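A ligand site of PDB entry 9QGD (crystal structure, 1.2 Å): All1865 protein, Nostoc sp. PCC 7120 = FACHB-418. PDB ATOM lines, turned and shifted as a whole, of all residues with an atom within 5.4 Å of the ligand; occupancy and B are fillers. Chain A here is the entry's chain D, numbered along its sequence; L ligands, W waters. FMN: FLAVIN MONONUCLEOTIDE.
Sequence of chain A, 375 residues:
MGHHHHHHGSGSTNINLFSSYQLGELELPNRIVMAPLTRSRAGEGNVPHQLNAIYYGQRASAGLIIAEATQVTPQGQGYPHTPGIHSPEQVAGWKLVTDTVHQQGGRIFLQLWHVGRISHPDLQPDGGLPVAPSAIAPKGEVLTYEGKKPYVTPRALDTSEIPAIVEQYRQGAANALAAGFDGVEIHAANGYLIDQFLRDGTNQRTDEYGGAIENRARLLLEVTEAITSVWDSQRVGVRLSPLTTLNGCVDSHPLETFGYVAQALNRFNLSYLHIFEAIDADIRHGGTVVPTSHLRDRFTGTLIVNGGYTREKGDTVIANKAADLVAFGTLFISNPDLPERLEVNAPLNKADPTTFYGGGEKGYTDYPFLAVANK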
ATOM      1  N   ALA A  35     -30.284  16.218   2.888  1.00  0.00           N
ATOM      2  CA  ALA A  35     -30.109  14.778   2.698  1.00  0.00           C
ATOM      3  C   ALA A  35     -29.194  14.237   3.794  1.00  0.00           C
ATOM      4  O   ALA A  35     -28.367  14.961   4.352  1.00  0.00           O
ATOM      5  CB  ALA A  35     -29.450  14.524   1.359  1.00  0.00           C
ATOM      6  N   PRO A  36     -29.292  12.921   4.075  1.00  0.00           N
ATOM      7  CA  PRO A  36     -28.398  12.302   5.037  1.00  0.00           C
ATOM      8  C   PRO A  36     -26.977  12.308   4.508  1.00  0.00           C
ATOM      9  O   PRO A  36     -26.695  11.946   3.375  1.00  0.00           O
ATOM     10  CB  PRO A  36     -28.961  10.873   5.174  1.00  0.00           C
ATOM     11  CG  PRO A  36     -29.704  10.608   3.842  1.00  0.00           C
ATOM     12  CD  PRO A  36     -30.241  11.983   3.422  1.00  0.00           C
ATOM     13  N   LEU A  37     -26.026  12.736   5.379  1.00  0.00           N
ATOM     14  CA  LEU A  37     -24.614  12.880   4.966  1.00  0.00           C
ATOM     15  C   LEU A  37     -23.697  12.374   6.083  1.00  0.00           C
ATOM     16  O   LEU A  37     -23.558  13.057   7.118  1.00  0.00           O
ATOM     17  CB  LEU A  37     -24.339  14.371   4.679  1.00  0.00           C
ATOM     18  CG  LEU A  37     -25.120  14.994   3.533  1.00  0.00           C
ATOM     19  CD1 LEU A  37     -25.216  16.509   3.776  1.00  0.00           C
ATOM     20  CD2 LEU A  37     -24.517  14.659   2.190  1.00  0.00           C
ATOM     21  N   THR A  38     -23.091  11.221   5.837  1.00  0.00           N
ATOM     22  CA  THR A  38     -22.055  10.694   6.708  1.00  0.00           C
ATOM     23  C   THR A  38     -20.910  11.709   6.753  1.00  0.00           C
ATOM     24  O   THR A  38     -20.344  12.066   5.717  1.00  0.00           O
ATOM     25  CB  THR A  38     -21.577   9.370   6.102  1.00  0.00           C
ATOM     26  OG1 THR A  38     -22.605   8.395   6.270  1.00  0.00           O
ATOM     27  CG2 THR A  38     -20.324   8.807   6.767  1.00  0.00           C
ATOM     28  N   ARG A  39     -20.546  12.138   7.984  1.00  0.00           N
ATOM     29  CA  ARG A  39     -19.425  13.068   8.160  1.00  0.00           C
ATOM     30  C   ARG A  39     -18.357  12.461   9.034  1.00  0.00           C
ATOM     31  O   ARG A  39     -17.297  13.086   9.201  1.00  0.00           O
ATOM     32  CB  ARG A  39     -19.932  14.370   8.745  1.00  0.00           C
ATOM     33  CG  ARG A  39     -21.083  15.020   7.977  1.00  0.00           C
ATOM     34  CD  ARG A  39     -20.829  15.302   6.498  1.00  0.00           C
ATOM     35  NE  ARG A  39     -19.589  16.071   6.307  1.00  0.00           N
ATOM     36  CZ  ARG A  39     -19.565  17.393   6.369  1.00  0.00           C
ATOM     37  NH1 ARG A  39     -20.644  18.146   6.612  1.00  0.00           N
ATOM     38  NH2 ARG A  39     -18.392  18.047   6.255  1.00  0.00           N
ATOM     39  N   GLU A  68     -27.361  12.029   9.289  1.00  0.00           N
ATOM     40  CA  GLU A  68     -26.426  11.055   8.718  1.00  0.00           C
ATOM     41  C   GLU A  68     -26.817   9.614   9.083  1.00  0.00           C
ATOM     42  O   GLU A  68     -27.326   9.332  10.170  1.00  0.00           O
ATOM     43  CB  GLU A  68     -25.022  11.336   9.250  1.00  0.00           C
ATOM     44  CG  GLU A  68     -24.866  11.089  10.758  1.00  0.00           C
ATOM     45  CD  GLU A  68     -23.759  11.926  11.368  1.00  0.00           C
ATOM     46  OE1 GLU A  68     -22.571  11.579  11.231  1.00  0.00           O
ATOM     47  OE2 GLU A  68     -24.074  13.055  11.909  1.00  0.00           O
ATOM     48  N   ALA A  69     -26.408   8.670   8.192  1.00  0.00           N
ATOM     49  CA  ALA A  69     -26.613   7.250   8.487  1.00  0.00           C
ATOM     50  C   ALA A  69     -26.014   6.906   9.839  1.00  0.00           C
ATOM     51  O   ALA A  69     -24.861   7.218  10.170  1.00  0.00           O
ATOM     52  CB  ALA A  69     -25.971   6.439   7.382  1.00  0.00           C
ATOM     53  N   GLN A 111     -31.502   8.828  10.145  1.00  0.00           N
ATOM     54  CA  GLN A 111     -31.365   7.737   9.203  1.00  0.00           C
ATOM     55  C   GLN A 111     -30.777   6.502   9.864  1.00  0.00           C
ATOM     56  O   GLN A 111     -29.663   6.554  10.422  1.00  0.00           O
ATOM     57  CB  GLN A 111     -30.581   8.167   7.990  1.00  0.00           C
ATOM     58  CG  GLN A 111     -30.697   7.109   6.870  1.00  0.00           C
ATOM     59  CD  GLN A 111     -29.779   7.316   5.699  1.00  0.00           C
ATOM     60  OE1 GLN A 111     -28.541   7.446   5.885  1.00  0.00           O
ATOM     61  NE2 GLN A 111     -30.309   7.310   4.488  1.00  0.00           N
ATOM     62  N   GLU A 185     -35.658   7.615   9.148  1.00  0.00           N
ATOM     63  CA  GLU A 185     -35.569   7.200   7.754  1.00  0.00           C
ATOM     64  C   GLU A 185     -34.873   5.846   7.726  1.00  0.00           C
ATOM     65  O   GLU A 185     -33.769   5.735   8.280  1.00  0.00           O
ATOM     66  CB  GLU A 185     -34.839   8.227   6.882  1.00  0.00           C
ATOM     67  CG  GLU A 185     -34.752   7.747   5.417  1.00  0.00           C
ATOM     68  CD  GLU A 185     -34.134   8.800   4.544  1.00  0.00           C
ATOM     69  OE1 GLU A 185     -32.902   8.659   4.285  1.00  0.00           O
ATOM     70  OE2 GLU A 185     -34.837   9.755   4.108  1.00  0.00           O
ATOM     71  N   HIS A 187     -32.575   3.410   5.937  1.00  0.00           N
ATOM     72  CA  HIS A 187     -31.617   3.442   4.847  1.00  0.00           C
ATOM     73  C   HIS A 187     -31.637   2.138   4.045  1.00  0.00           C
ATOM     74  O   HIS A 187     -31.051   1.122   4.447  1.00  0.00           O
ATOM     75  CB  HIS A 187     -30.214   3.680   5.405  1.00  0.00           C
ATOM     76  CG  HIS A 187     -29.211   4.030   4.346  1.00  0.00           C
ATOM     77  ND1 HIS A 187     -27.944   4.579   4.476  1.00  0.00           N
ATOM     78  CD2 HIS A 187     -29.460   3.878   3.001  1.00  0.00           C
ATOM     79  CE1 HIS A 187     -27.469   4.812   3.242  1.00  0.00           C
ATOM     80  NE2 HIS A 187     -28.403   4.388   2.339  1.00  0.00           N
ATOM     81  N   ALA A 189     -30.828   2.029   0.806  1.00  0.00           N
ATOM     82  CA  ALA A 189     -30.164   2.527  -0.397  1.00  0.00           C
ATOM     83  C   ALA A 189     -28.656   2.258  -0.322  1.00  0.00           C
ATOM     84  O   ALA A 189     -28.140   1.642   0.640  1.00  0.00           O
ATOM     85  CB  ALA A 189     -30.402   3.997  -0.576  1.00  0.00           C
ATOM     86  N   ASN A 190     -27.965   2.640  -1.406  1.00  0.00           N
ATOM     87  CA  ASN A 190     -26.508   2.768  -1.487  1.00  0.00           C
ATOM     88  C   ASN A 190     -25.795   1.456  -1.226  1.00  0.00           C
ATOM     89  O   ASN A 190     -24.600   1.471  -0.903  1.00  0.00           O
ATOM     90  CB  ASN A 190     -25.990   3.902  -0.646  1.00  0.00           C
ATOM     91  CG  ASN A 190     -26.544   5.217  -1.111  1.00  0.00           C
ATOM     92  OD1 ASN A 190     -27.089   5.298  -2.235  1.00  0.00           O
ATOM     93  ND2 ASN A 190     -26.468   6.269  -0.280  1.00  0.00           N
ATOM     94  N   ARG A 239     -35.571   5.231   2.277  1.00  0.00           N
ATOM     95  CA  ARG A 239     -34.772   5.734   1.169  1.00  0.00           C
ATOM     96  C   ARG A 239     -34.337   4.570   0.281  1.00  0.00           C
ATOM     97  O   ARG A 239     -33.864   3.548   0.784  1.00  0.00           O
ATOM     98  CB  ARG A 239     -33.516   6.432   1.711  1.00  0.00           C
ATOM     99  CG  ARG A 239     -32.898   7.287   0.599  1.00  0.00           C
ATOM    100  CD  ARG A 239     -31.732   8.101   1.115  1.00  0.00           C
ATOM    101  NE  ARG A 239     -31.567   9.262   0.217  1.00  0.00           N
ATOM    102  CZ  ARG A 239     -30.459  10.001   0.046  1.00  0.00           C
ATOM    103  NH1 ARG A 239     -29.275   9.557   0.435  1.00  0.00           N
ATOM    104  NH2 ARG A 239     -30.517  11.187  -0.545  1.00  0.00           N
ATOM    105  N   PHE A 276     -32.907   8.608  -4.072  1.00  0.00           N
ATOM    106  CA  PHE A 276     -31.631   9.148  -4.551  1.00  0.00           C
ATOM    107  C   PHE A 276     -31.486   8.705  -6.011  1.00  0.00           C
ATOM    108  O   PHE A 276     -31.349   7.500  -6.276  1.00  0.00           O
ATOM    109  CB  PHE A 276     -30.533   8.581  -3.666  1.00  0.00           C
ATOM    110  CG  PHE A 276     -29.119   8.840  -4.121  1.00  0.00           C
ATOM    111  CD1 PHE A 276     -28.797   9.810  -5.076  1.00  0.00           C
ATOM    112  CD2 PHE A 276     -28.121   8.082  -3.509  1.00  0.00           C
ATOM    113  CE1 PHE A 276     -27.437   9.999  -5.417  1.00  0.00           C
ATOM    114  CE2 PHE A 276     -26.788   8.255  -3.859  1.00  0.00           C
ATOM    115  CZ  PHE A 276     -26.464   9.205  -4.829  1.00  0.00           C
ATOM    116  N   ILE A 279     -26.384  10.048 -10.053  1.00  0.00           N
ATOM    117  CA  ILE A 279     -25.956  11.173 -10.875  1.00  0.00           C
ATOM    118  C   ILE A 279     -25.583  10.684 -12.278  1.00  0.00           C
ATOM    119  O   ILE A 279     -25.708  11.413 -13.259  1.00  0.00           O
ATOM    120  CB  ILE A 279     -24.784  11.943 -10.176  1.00  0.00           C
ATOM    121  CG1 ILE A 279     -25.284  12.548  -8.881  1.00  0.00           C
ATOM    122  CG2 ILE A 279     -24.059  12.919 -11.076  1.00  0.00           C
ATOM    123  CD1 ILE A 279     -26.633  13.221  -9.048  1.00  0.00           C
ATOM    124  N   ASN A 306     -33.817  13.432  -5.004  1.00  0.00           N
ATOM    125  CA  ASN A 306     -32.512  13.904  -4.648  1.00  0.00           C
ATOM    126  C   ASN A 306     -31.557  13.503  -5.763  1.00  0.00           C
ATOM    127  O   ASN A 306     -31.693  12.461  -6.383  1.00  0.00           O
ATOM    128  CB  ASN A 306     -32.073  13.216  -3.339  1.00  0.00           C
ATOM    129  CG  ASN A 306     -30.581  13.254  -3.118  1.00  0.00           C
ATOM    130  OD1 ASN A 306     -29.900  12.299  -3.514  1.00  0.00           O
ATOM    131  ND2 ASN A 306     -30.064  14.369  -2.625  1.00  0.00           N
ATOM    132  N   GLY A 307     -30.472  14.316  -5.929  1.00  0.00           N
ATOM    133  CA  GLY A 307     -29.332  13.939  -6.773  1.00  0.00           C
ATOM    134  C   GLY A 307     -29.058  15.036  -7.772  1.00  0.00           C
ATOM    135  O   GLY A 307     -29.734  15.127  -8.790  1.00  0.00           O
ATOM    136  N   GLY A 308     -28.109  15.928  -7.435  1.00  0.00           N
ATOM    137  CA  GLY A 308     -27.767  16.981  -8.386  1.00  0.00           C
ATOM    138  C   GLY A 308     -28.839  18.059  -8.557  1.00  0.00           C
ATOM    139  O   GLY A 308     -28.805  18.814  -9.521  1.00  0.00           O
ATOM    140  N   TYR A 309     -29.720  18.250  -7.576  1.00  0.00           N
ATOM    141  CA  TYR A 309     -30.734  19.301  -7.690  1.00  0.00           C
ATOM    142  C   TYR A 309     -30.183  20.705  -7.515  1.00  0.00           C
ATOM    143  O   TYR A 309     -29.183  20.932  -6.843  1.00  0.00           O
ATOM    144  CB  TYR A 309     -31.954  19.056  -6.784  1.00  0.00           C
ATOM    145  CG  TYR A 309     -32.844  18.016  -7.429  1.00  0.00           C
ATOM    146  CD1 TYR A 309     -32.564  16.666  -7.280  1.00  0.00           C
ATOM    147  CD2 TYR A 309     -33.915  18.411  -8.230  1.00  0.00           C
ATOM    148  CE1 TYR A 309     -33.303  15.705  -7.960  1.00  0.00           C
ATOM    149  CE2 TYR A 309     -34.698  17.449  -8.873  1.00  0.00           C
ATOM    150  CZ  TYR A 309     -34.366  16.102  -8.756  1.00  0.00           C
ATOM    151  OH  TYR A 309     -35.172  15.186  -9.403  1.00  0.00           O
ATOM    152  N   ALA A 327     -34.357  16.906  -1.647  1.00  0.00           N
ATOM    153  CA  ALA A 327     -33.248  16.884  -0.701  1.00  0.00           C
ATOM    154  C   ALA A 327     -31.962  17.246  -1.424  1.00  0.00           C
ATOM    155  O   ALA A 327     -31.675  16.825  -2.558  1.00  0.00           O
ATOM    156  CB  ALA A 327     -33.181  15.455  -0.107  1.00  0.00           C
ATOM    157  N   PHE A 328     -31.135  18.002  -0.692  1.00  0.00           N
ATOM    158  CA  PHE A 328     -29.817  18.456  -1.157  1.00  0.00           C
ATOM    159  C   PHE A 328     -28.782  17.905  -0.189  1.00  0.00           C
ATOM    160  O   PHE A 328     -28.956  18.048   1.032  1.00  0.00           O
ATOM    161  CB  PHE A 328     -29.760  19.985  -1.157  1.00  0.00           C
ATOM    162  CG  PHE A 328     -30.748  20.644  -2.116  1.00  0.00           C
ATOM    163  CD1 PHE A 328     -32.091  20.832  -1.745  1.00  0.00           C
ATOM    164  CD2 PHE A 328     -30.302  21.061  -3.373  1.00  0.00           C
ATOM    165  CE1 PHE A 328     -32.974  21.472  -2.630  1.00  0.00           C
ATOM    166  CE2 PHE A 328     -31.193  21.717  -4.231  1.00  0.00           C
ATOM    167  CZ  PHE A 328     -32.518  21.910  -3.851  1.00  0.00           C
ATOM    168  N   GLY A 329     -27.784  17.270  -0.771  1.00  0.00           N
ATOM    169  CA  GLY A 329     -26.694  16.743   0.043  1.00  0.00           C
ATOM    170  C   GLY A 329     -25.490  17.700   0.014  1.00  0.00           C
ATOM    171  O   GLY A 329     -25.300  18.492   0.922  1.00  0.00           O
ATOM    172  N   THR A 330     -24.739  17.634  -1.098  1.00  0.00           N
ATOM    173  CA  THR A 330     -23.489  18.407  -1.201  1.00  0.00           C
ATOM    174  C   THR A 330     -23.725  19.874  -0.851  1.00  0.00           C
ATOM    175  O   THR A 330     -22.916  20.465  -0.127  1.00  0.00           O
ATOM    176  CB  THR A 330     -22.979  18.269  -2.650  1.00  0.00           C
ATOM    177  OG1 THR A 330     -22.763  16.885  -2.900  1.00  0.00           O
ATOM    178  CG2 THR A 330     -21.681  19.010  -2.823  1.00  0.00           C
ATOM    179  N   LEU A 331     -24.788  20.516  -1.370  1.00  0.00           N
ATOM    180  CA  LEU A 331     -24.940  21.948  -1.131  1.00  0.00           C
ATOM    181  C   LEU A 331     -25.204  22.253   0.340  1.00  0.00           C
ATOM    182  O   LEU A 331     -24.873  23.342   0.796  1.00  0.00           O
ATOM    183  CB  LEU A 331     -26.047  22.542  -2.012  1.00  0.00           C
ATOM    184  CG  LEU A 331     -25.665  22.751  -3.451  1.00  0.00           C
ATOM    185  CD1 LEU A 331     -26.905  23.217  -4.240  1.00  0.00           C
ATOM    186  CD2 LEU A 331     -24.513  23.780  -3.617  1.00  0.00           C
ATOM    187  N   ILE A 333     -23.724  20.624   2.764  1.00  0.00           N
ATOM    188  CA  ILE A 333     -22.436  20.577   3.441  1.00  0.00           C
ATOM    189  C   ILE A 333     -21.874  21.996   3.503  1.00  0.00           C
ATOM    190  O   ILE A 333     -21.452  22.472   4.582  1.00  0.00           O
ATOM    191  CB  ILE A 333     -21.466  19.652   2.698  1.00  0.00           C
ATOM    192  CG1 ILE A 333     -21.928  18.196   2.815  1.00  0.00           C
ATOM    193  CG2 ILE A 333     -20.048  19.815   3.286  1.00  0.00           C
ATOM    194  CD1 ILE A 333     -21.067  17.221   2.038  1.00  0.00           C
ATOM    195  N   PHE A 356     -14.989  16.258   3.921  1.00  0.00           N
ATOM    196  CA  PHE A 356     -16.269  15.602   4.082  1.00  0.00           C
ATOM    197  C   PHE A 356     -16.256  14.662   5.290  1.00  0.00           C
ATOM    198  O   PHE A 356     -17.236  14.601   6.051  1.00  0.00           O
ATOM    199  CB  PHE A 356     -16.734  14.828   2.851  1.00  0.00           C
ATOM    200  CG  PHE A 356     -17.168  15.707   1.691  1.00  0.00           C
ATOM    201  CD1 PHE A 356     -17.257  17.112   1.786  1.00  0.00           C
ATOM    202  CD2 PHE A 356     -17.548  15.085   0.485  1.00  0.00           C
ATOM    203  CE1 PHE A 356     -17.695  17.879   0.692  1.00  0.00           C
ATOM    204  CE2 PHE A 356     -17.939  15.859  -0.593  1.00  0.00           C
ATOM    205  CZ  PHE A 356     -18.031  17.240  -0.500  1.00  0.00           C
ATOM    206  N   TYR A 357     -15.182  13.881   5.433  1.00  0.00           N
ATOM    207  CA  TYR A 357     -15.178  12.806   6.428  1.00  0.00           C
ATOM    208  C   TYR A 357     -14.082  13.015   7.471  1.00  0.00           C
ATOM    209  O   TYR A 357     -12.911  13.265   7.162  1.00  0.00           O
ATOM    210  CB  TYR A 357     -14.878  11.502   5.708  1.00  0.00           C
ATOM    211  CG  TYR A 357     -15.901  11.180   4.636  1.00  0.00           C
ATOM    212  CD1 TYR A 357     -17.198  10.833   4.967  1.00  0.00           C
ATOM    213  CD2 TYR A 357     -15.554  11.202   3.272  1.00  0.00           C
ATOM    214  CE1 TYR A 357     -18.128  10.512   4.003  1.00  0.00           C
ATOM    215  CE2 TYR A 357     -16.464  10.847   2.289  1.00  0.00           C
ATOM    216  CZ  TYR A 357     -17.757  10.516   2.669  1.00  0.00           C
ATOM    217  OH  TYR A 357     -18.658  10.171   1.686  1.00  0.00           O
HETATM  218  N1  FMN L   1     -26.658   8.943   1.558  1.00  0.00           N
HETATM  219  C2  FMN L   1     -27.299   8.337   2.541  1.00  0.00           C
HETATM  220  O2  FMN L   1     -28.381   7.729   2.361  1.00  0.00           O
HETATM  221  N3  FMN L   1     -26.790   8.299   3.833  1.00  0.00           N
HETATM  222  C4  FMN L   1     -25.561   8.866   4.131  1.00  0.00           C
HETATM  223  O4  FMN L   1     -25.201   8.880   5.325  1.00  0.00           O
HETATM  224  C4A FMN L   1     -24.841   9.461   3.075  1.00  0.00           C
HETATM  225  N5  FMN L   1     -23.631   9.997   3.337  1.00  0.00           N
HETATM  226  C5A FMN L   1     -23.083  10.822   2.387  1.00  0.00           C
HETATM  227  C6  FMN L   1     -21.907  11.531   2.684  1.00  0.00           C
HETATM  228  C7  FMN L   1     -21.359  12.394   1.779  1.00  0.00           C
HETATM  229  C7M FMN L   1     -20.115  13.152   2.164  1.00  0.00           C
HETATM  230  C8  FMN L   1     -21.967  12.576   0.506  1.00  0.00           C
HETATM  231  C8M FMN L   1     -21.409  13.565  -0.482  1.00  0.00           C
HETATM  232  C9  FMN L   1     -23.111  11.850   0.202  1.00  0.00           C
HETATM  233  C9A FMN L   1     -23.684  10.980   1.133  1.00  0.00           C
HETATM  234  N10 FMN L   1     -24.879  10.278   0.846  1.00  0.00           N
HETATM  235  C10 FMN L   1     -25.516   9.524   1.813  1.00  0.00           C
HETATM  236  C1' FMN L   1     -25.614  10.544  -0.391  1.00  0.00           C
HETATM  237  C2' FMN L   1     -26.326  11.904  -0.295  1.00  0.00           C
HETATM  238  O2' FMN L   1     -27.392  11.863   0.695  1.00  0.00           O
HETATM  239  C3' FMN L   1     -26.974  12.379  -1.584  1.00  0.00           C
HETATM  240  O3' FMN L   1     -27.967  11.378  -1.912  1.00  0.00           O
HETATM  241  C4' FMN L   1     -25.996  12.501  -2.755  1.00  0.00           C
HETATM  242  O4' FMN L   1     -24.833  13.243  -2.323  1.00  0.00           O
HETATM  243  C5' FMN L   1     -26.622  13.134  -3.973  1.00  0.00           C
HETATM  244  O5' FMN L   1     -27.276  14.391  -3.633  1.00  0.00           O
HETATM  245  P   FMN L   1     -26.542  15.786  -3.955  1.00  0.00           P
HETATM  246  O1P FMN L   1     -27.544  16.791  -3.493  1.00  0.00           O
HETATM  247  O2P FMN L   1     -26.246  15.801  -5.393  1.00  0.00           O
HETATM  248  O3P FMN L   1     -25.308  15.842  -3.105  1.00  0.00           O
HETATM  249  O   HOH W   1     -26.743  19.472  -3.258  1.00  0.00           O
HETATM  250  O   HOH W   2     -25.104  18.059  -6.472  1.00  0.00           O
HETATM  251  O   HOH W   3     -29.954  16.926  -4.806  1.00  0.00           O
HETATM  252  O   HOH W   4     -24.012  14.608  -6.431  1.00  0.00           O
HETATM  253  O   HOH W   5     -22.886  11.941  -3.724  1.00  0.00           O
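OD1 of Asn 306 is in hydrogen-bond range of O3' of the ligand (2.7 Å). The backbone NH (N) of Thr 330 is in hydrogen-bond range of an oxygen (O3P) of the ligand (2.8 Å). The side-chain hydroxyl of Thr 330 lies within hydrogen-bond range of an oxygen (O3P) of the ligand, 2.8 Å away. An oxygen (O2P) of the ligand is in hydrogen-bond range of the backbone NH of Gly 308, at 2.8 Å. The backbone carbonyl oxygen (O) of Pro 36 lies within hydrogen-bond range of an oxygen (O2') of the ligand (2.8 Å). The backbone NH (N) of Gly 329 sits at hydrogen-bond distance from an oxygen (O1P) of the ligand, 2.8 Å away. The guanidinium group (NH1) of Arg 239 sits at hydrogen-bond distance from an oxygen (O2) of the ligand (2.8 Å). A nitrogen (N5) of the ligand is in hydrogen-bond range of the backbone NH of Thr 38. OG1 of Thr 38 sits at hydrogen-bond distance from O4 of the ligand (2.8 Å). OE1 of Gln 111 lies within hydrogen-bond range of N3 of the ligand (2.8 Å). An oxygen (O4) of the ligand lies within hydrogen-bond range of the backbone NH (N) of Ala 69, at 3.1 Å. A ring nitrogen (NE2) of His 187 lies close to an oxygen (O2) of the ligand. A nitrogen (N1) of the ligand sits at hydrogen-bond distance from the side-chain amide nitrogen (ND2) of Asn 190, 3.3 Å away.
OD1 of Asn 306 is in hydrogen-bond range of NH2 of Arg 239. O of Arg 239 is in hydrogen-bond range of N of Ala 189 (3.4 Å). The side-chain amide oxygen (OE1) of Gln 111 sits close to the backbone NH (N) of Ala 69. The side-chain amide oxygen of Gln 111 is in hydrogen-bond range of a ring nitrogen (ND1) of His 187, at 3.2 Å. The side-chain carboxylate (OE1) of Glu 185 is in hydrogen-bond range of the side-chain amide nitrogen (NE2) of Gln 111, at 2.9 Å. A ring nitrogen (NE2) of His 187 lies within hydrogen-bond range of the backbone carbonyl oxygen (O) of Ala 189 (3.2 Å). The backbone NH (N) of Ala 35 lies within hydrogen-bond range of the backbone carbonyl oxygen (O) of Phe 328 (2.9 Å). The guanidinium group (NE) of Arg 39 lies within hydrogen-bond range of the backbone carbonyl oxygen (O) of Phe 356, at 2.8 Å.
Merely in contact with the ligand: Ala 35 (3.4 Å), Leu 37 (3.5 Å), Phe 276 (3.5 Å), Gly 307 (3.8 Å), Phe 328 (3.7 Å), Phe 356 (3.6 Å) and Tyr 357 (3.4 Å). Hydrophobic or aromatic side chains within 4 Å of the ligand: Ala 35, Pro 36, Leu 37, Ala 69, His 187, Phe 276, Phe 356 and Tyr 357. The nearest printed residue that does not touch the ligand is Glu 68 (4.2 Å).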
